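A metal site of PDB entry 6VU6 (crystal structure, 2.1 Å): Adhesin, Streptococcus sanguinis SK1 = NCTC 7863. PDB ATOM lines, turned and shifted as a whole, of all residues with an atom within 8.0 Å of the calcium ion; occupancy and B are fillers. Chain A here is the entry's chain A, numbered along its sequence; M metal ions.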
ATOM      1  N   THR A   1      27.883 -18.759  -6.996  1.00  0.00           N
ATOM      2  CA  THR A   1      26.566 -18.596  -7.655  1.00  0.00           C
ATOM      3  C   THR A   1      26.794 -18.186  -9.106  1.00  0.00           C
ATOM      4  O   THR A   1      27.693 -17.451  -9.352  1.00  0.00           O
ATOM      5  CB  THR A   1      25.789 -17.378  -7.159  1.00  0.00           C
ATOM      6  OG1 THR A   1      26.548 -16.553  -6.274  1.00  0.00           O
ATOM      7  CG2 THR A   1      24.407 -17.730  -6.652  1.00  0.00           C
ATOM      8  N   ASP A   2      25.948 -18.664 -10.001  1.00  0.00           N
ATOM      9  CA  ASP A   2      25.990 -18.306 -11.433  1.00  0.00           C
ATOM     10  C   ASP A   2      25.620 -16.840 -11.494  1.00  0.00           C
ATOM     11  O   ASP A   2      24.548 -16.520 -11.095  1.00  0.00           O
ATOM     12  CB  ASP A   2      25.002 -19.142 -12.234  1.00  0.00           C
ATOM     13  CG  ASP A   2      25.011 -18.778 -13.701  1.00  0.00           C
ATOM     14  OD1 ASP A   2      25.442 -17.713 -14.020  1.00  0.00           O
ATOM     15  OD2 ASP A   2      24.601 -19.574 -14.486  1.00  0.00           O
ATOM     16  N   THR A   3      26.508 -15.988 -11.941  1.00  0.00           N
ATOM     17  CA  THR A   3      26.184 -14.553 -12.022  1.00  0.00           C
ATOM     18  C   THR A   3      26.335 -14.054 -13.464  1.00  0.00           C
ATOM     19  O   THR A   3      26.320 -12.878 -13.678  1.00  0.00           O
ATOM     20  CB  THR A   3      27.107 -13.802 -11.079  1.00  0.00           C
ATOM     21  OG1 THR A   3      28.431 -13.857 -11.595  1.00  0.00           O
ATOM     22  CG2 THR A   3      27.093 -14.392  -9.696  1.00  0.00           C
ATOM     23  N   THR A   4      26.420 -14.952 -14.417  1.00  0.00           N
ATOM     24  CA  THR A   4      26.699 -14.598 -15.818  1.00  0.00           C
ATOM     25  C   THR A   4      25.471 -14.809 -16.687  1.00  0.00           C
ATOM     26  O   THR A   4      24.928 -15.822 -16.615  1.00  0.00           O
ATOM     27  CB  THR A   4      27.855 -15.474 -16.290  1.00  0.00           C
ATOM     28  OG1 THR A   4      28.914 -15.001 -15.482  1.00  0.00           O
ATOM     29  CG2 THR A   4      28.219 -15.285 -17.742  1.00  0.00           C
ATOM     30  N   PRO A   5      25.049 -13.893 -17.568  1.00  0.00           N
ATOM     31  CA  PRO A   5      23.897 -14.176 -18.408  1.00  0.00           C
ATOM     32  C   PRO A   5      24.275 -15.070 -19.590  1.00  0.00           C
ATOM     33  O   PRO A   5      25.347 -15.247 -19.857  1.00  0.00           O
ATOM     34  CB  PRO A   5      23.544 -12.798 -18.929  1.00  0.00           C
ATOM     35  CG  PRO A   5      24.839 -12.068 -18.928  1.00  0.00           C
ATOM     36  CD  PRO A   5      25.684 -12.641 -17.816  1.00  0.00           C
ATOM     37  N   PRO A   6      23.329 -15.605 -20.334  1.00  0.00           N
ATOM     38  CA  PRO A   6      23.640 -16.389 -21.509  1.00  0.00           C
ATOM     39  C   PRO A   6      24.228 -15.586 -22.689  1.00  0.00           C
ATOM     40  O   PRO A   6      24.252 -14.431 -22.716  1.00  0.00           O
ATOM     41  CB  PRO A   6      22.285 -16.963 -21.902  1.00  0.00           C
ATOM     42  CG  PRO A   6      21.463 -16.844 -20.694  1.00  0.00           C
ATOM     43  CD  PRO A   6      21.924 -15.567 -20.083  1.00  0.00           C
ATOM     44  N   THR A   7      24.731 -16.336 -23.631  1.00  0.00           N
ATOM     45  CA  THR A   7      25.323 -15.848 -24.902  1.00  0.00           C
ATOM     46  C   THR A   7      24.292 -16.111 -25.989  1.00  0.00           C
ATOM     47  O   THR A   7      23.814 -17.179 -26.016  1.00  0.00           O
ATOM     48  CB  THR A   7      26.590 -16.658 -25.179  1.00  0.00           C
ATOM     49  OG1 THR A   7      27.564 -16.355 -24.207  1.00  0.00           O
ATOM     50  CG2 THR A   7      27.146 -16.438 -26.559  1.00  0.00           C
ATOM     51  N   THR A  29      23.417 -20.135 -25.601  1.00  0.00           N
ATOM     52  CA  THR A  29      24.087 -21.045 -24.670  1.00  0.00           C
ATOM     53  C   THR A  29      24.277 -20.346 -23.321  1.00  0.00           C
ATOM     54  O   THR A  29      24.237 -19.152 -23.287  1.00  0.00           O
ATOM     55  CB  THR A  29      25.439 -21.502 -25.209  1.00  0.00           C
ATOM     56  OG1 THR A  29      26.264 -20.370 -25.058  1.00  0.00           O
ATOM     57  CG2 THR A  29      25.430 -21.825 -26.681  1.00  0.00           C
ATOM     58  N   ASP A  30      24.512 -21.105 -22.249  1.00  0.00           N
ATOM     59  CA  ASP A  30      24.874 -20.586 -20.900  1.00  0.00           C
ATOM     60  C   ASP A  30      25.919 -21.529 -20.272  1.00  0.00           C
ATOM     61  O   ASP A  30      25.839 -22.652 -20.491  1.00  0.00           O
ATOM     62  CB  ASP A  30      23.674 -20.336 -19.980  1.00  0.00           C
ATOM     63  CG  ASP A  30      23.969 -19.565 -18.718  1.00  0.00           C
ATOM     64  OD1 ASP A  30      24.174 -18.391 -18.816  1.00  0.00           O
ATOM     65  OD2 ASP A  30      23.997 -20.127 -17.664  1.00  0.00           O
ATOM     66  N   ASP A  31      26.800 -20.950 -19.459  1.00  0.00           N
ATOM     67  CA  ASP A  31      27.883 -21.580 -18.654  1.00  0.00           C
ATOM     68  C   ASP A  31      27.300 -22.711 -17.808  1.00  0.00           C
ATOM     69  O   ASP A  31      27.957 -23.681 -17.678  1.00  0.00           O
ATOM     70  CB  ASP A  31      28.636 -20.548 -17.785  1.00  0.00           C
ATOM     71  CG  ASP A  31      27.791 -19.785 -16.761  1.00  0.00           C
ATOM     72  OD1 ASP A  31      26.851 -19.086 -17.151  1.00  0.00           O
ATOM     73  OD2 ASP A  31      28.091 -19.861 -15.570  1.00  0.00           O
ATOM     74  N   SER A  32      26.085 -22.528 -17.281  1.00  0.00           N
ATOM     75  CA  SER A  32      25.360 -23.519 -16.450  1.00  0.00           C
ATOM     76  C   SER A  32      24.727 -24.605 -17.308  1.00  0.00           C
ATOM     77  O   SER A  32      24.244 -25.526 -16.728  1.00  0.00           O
ATOM     78  CB  SER A  32      24.304 -22.840 -15.650  1.00  0.00           C
ATOM     79  OG  SER A  32      23.080 -22.773 -16.373  1.00  0.00           O
ATOM     80  N   GLY A  33      24.601 -24.403 -18.613  1.00  0.00           N
ATOM     81  CA  GLY A  33      23.970 -25.372 -19.508  1.00  0.00           C
ATOM     82  C   GLY A  33      22.463 -25.313 -19.530  1.00  0.00           C
ATOM     83  O   GLY A  33      21.893 -26.079 -20.239  1.00  0.00           O
ATOM     84  N   ARG A  34      21.834 -24.416 -18.782  1.00  0.00           N
ATOM     85  CA  ARG A  34      20.354 -24.380 -18.783  1.00  0.00           C
ATOM     86  C   ARG A  34      19.861 -22.966 -19.066  1.00  0.00           C
ATOM     87  O   ARG A  34      20.386 -22.044 -18.468  1.00  0.00           O
ATOM     88  CB  ARG A  34      19.787 -24.791 -17.426  1.00  0.00           C
ATOM     89  CG  ARG A  34      18.265 -24.877 -17.380  1.00  0.00           C
ATOM     90  CD  ARG A  34      17.651 -25.321 -16.057  1.00  0.00           C
ATOM     91  NE  ARG A  34      16.240 -25.023 -15.914  1.00  0.00           N
ATOM     92  CZ  ARG A  34      15.434 -25.558 -15.009  1.00  0.00           C
ATOM     93  NH1 ARG A  34      15.931 -26.427 -14.151  1.00  0.00           N
ATOM     94  NH2 ARG A  34      14.173 -25.230 -14.951  1.00  0.00           N
ATOM     95  N   VAL A  35      18.853 -22.844 -19.932  1.00  0.00           N
ATOM     96  CA  VAL A  35      18.250 -21.507 -20.163  1.00  0.00           C
ATOM     97  C   VAL A  35      16.752 -21.635 -19.943  1.00  0.00           C
ATOM     98  O   VAL A  35      16.170 -22.513 -20.494  1.00  0.00           O
ATOM     99  CB  VAL A  35      18.598 -20.977 -21.570  1.00  0.00           C
ATOM    100  CG1 VAL A  35      17.556 -20.019 -22.096  1.00  0.00           C
ATOM    101  CG2 VAL A  35      19.948 -20.349 -21.558  1.00  0.00           C
ATOM    102  N   GLU A 103      17.325 -15.675 -20.505  1.00  0.00           N
ATOM    103  CA  GLU A 103      17.449 -15.739 -19.038  1.00  0.00           C
ATOM    104  C   GLU A 103      17.807 -17.163 -18.607  1.00  0.00           C
ATOM    105  O   GLU A 103      17.115 -18.068 -18.930  1.00  0.00           O
ATOM    106  CB  GLU A 103      16.165 -15.331 -18.351  1.00  0.00           C
ATOM    107  CG  GLU A 103      16.347 -15.001 -16.904  1.00  0.00           C
ATOM    108  CD  GLU A 103      15.058 -14.968 -16.114  1.00  0.00           C
ATOM    109  OE1 GLU A 103      14.802 -15.929 -15.365  1.00  0.00           O
ATOM    110  OE2 GLU A 103      14.311 -14.002 -16.244  1.00  0.00           O
ATOM    111  N   ASP A 104      18.810 -17.306 -17.763  1.00  0.00           N
ATOM    112  CA  ASP A 104      19.171 -18.655 -17.300  1.00  0.00           C
ATOM    113  C   ASP A 104      18.314 -19.081 -16.107  1.00  0.00           C
ATOM    114  O   ASP A 104      17.492 -18.358 -15.666  1.00  0.00           O
ATOM    115  CB  ASP A 104      20.648 -18.768 -16.953  1.00  0.00           C
ATOM    116  CG  ASP A 104      21.148 -17.750 -15.966  1.00  0.00           C
ATOM    117  OD1 ASP A 104      20.408 -17.293 -15.123  1.00  0.00           O
ATOM    118  OD2 ASP A 104      22.289 -17.425 -16.053  1.00  0.00           O
ATOM    119  N   ALA A 105      18.671 -20.220 -15.537  1.00  0.00           N
ATOM    120  CA  ALA A 105      17.899 -20.828 -14.433  1.00  0.00           C
ATOM    121  C   ALA A 105      18.165 -20.134 -13.117  1.00  0.00           C
ATOM    122  O   ALA A 105      17.446 -20.437 -12.220  1.00  0.00           O
ATOM    123  CB  ALA A 105      18.168 -22.295 -14.312  1.00  0.00           C
ATOM    124  N   ALA A 106      19.180 -19.307 -13.022  1.00  0.00           N
ATOM    125  CA  ALA A 106      19.473 -18.599 -11.762  1.00  0.00           C
ATOM    126  C   ALA A 106      18.964 -17.163 -11.850  1.00  0.00           C
ATOM    127  O   ALA A 106      19.152 -16.432 -10.929  1.00  0.00           O
ATOM    128  CB  ALA A 106      20.938 -18.667 -11.527  1.00  0.00           C
ATOM    129  N   GLY A 107      18.332 -16.811 -12.975  1.00  0.00           N
ATOM    130  CA  GLY A 107      17.762 -15.463 -13.133  1.00  0.00           C
ATOM    131  C   GLY A 107      18.607 -14.441 -13.867  1.00  0.00           C
ATOM    132  O   GLY A 107      18.168 -13.344 -13.954  1.00  0.00           O
ATOM    133  N   ASN A 108      19.781 -14.782 -14.371  1.00  0.00           N
ATOM    134  CA  ASN A 108      20.589 -13.772 -15.089  1.00  0.00           C
ATOM    135  C   ASN A 108      20.003 -13.534 -16.486  1.00  0.00           C
ATOM    136  O   ASN A 108      19.930 -14.485 -17.237  1.00  0.00           O
ATOM    137  CB  ASN A 108      22.064 -14.164 -15.100  1.00  0.00           C
ATOM    138  CG  ASN A 108      22.597 -14.534 -13.727  1.00  0.00           C
ATOM    139  OD1 ASN A 108      22.712 -13.702 -12.855  1.00  0.00           O
ATOM    140  ND2 ASN A 108      22.938 -15.780 -13.544  1.00  0.00           N
ATOM    141  N   ILE A 109      19.601 -12.316 -16.809  1.00  0.00           N
ATOM    142  CA  ILE A 109      19.015 -12.003 -18.136  1.00  0.00           C
ATOM    143  C   ILE A 109      19.997 -11.166 -18.935  1.00  0.00           C
ATOM    144  O   ILE A 109      20.632 -10.349 -18.392  1.00  0.00           O
ATOM    145  CB  ILE A 109      17.639 -11.306 -18.059  1.00  0.00           C
ATOM    146  CG1 ILE A 109      16.889 -11.347 -19.389  1.00  0.00           C
ATOM    147  CG2 ILE A 109      17.764  -9.879 -17.541  1.00  0.00           C
ATOM    148  CD1 ILE A 109      15.575 -10.663 -19.429  1.00  0.00           C
HETATM  149 CA    CA M   1      24.800 -18.292 -16.354  1.00  0.00          CA
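O of Asp 2 lies within hydrogen-bond range of ND2 of Asn 108 (3.0 Å).
The side-chain carboxylate of Asp 104 sits at hydrogen-bond distance from the backbone NH of Asn 108.
OD2 of Asp 30 lies close to OG of Ser 32, at 3.1 Å.
The backbone NH of Ala 106 lies within hydrogen-bond range of the side-chain carboxylate of Asp 104.
The backbone NH (N) of Gly 107 sits at hydrogen-bond distance from the side-chain carboxylate (OD1) of Asp 104, 3.0 Å away.
Of the 21 residues printed, 5 come within 4 Å of the calcium ion.
The calcium ion is bound by OD2 of Asp 2 (2.3 Å).
OD1 of Asp 31 binds the calcium ion (2.3 Å).
OD2 of Asp 30 is bound to the calcium ion (2.4 Å).
O of Thr 4 is bound to the calcium ion (2.5 Å).
The calcium ion is bound by OD1 of Asp 2, at 2.5 Å.
The calcium ion is bound by OD1 of Asp 30 (2.5 Å).
OD2 of Asp 104 is bound to the calcium ion (2.7 Å).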
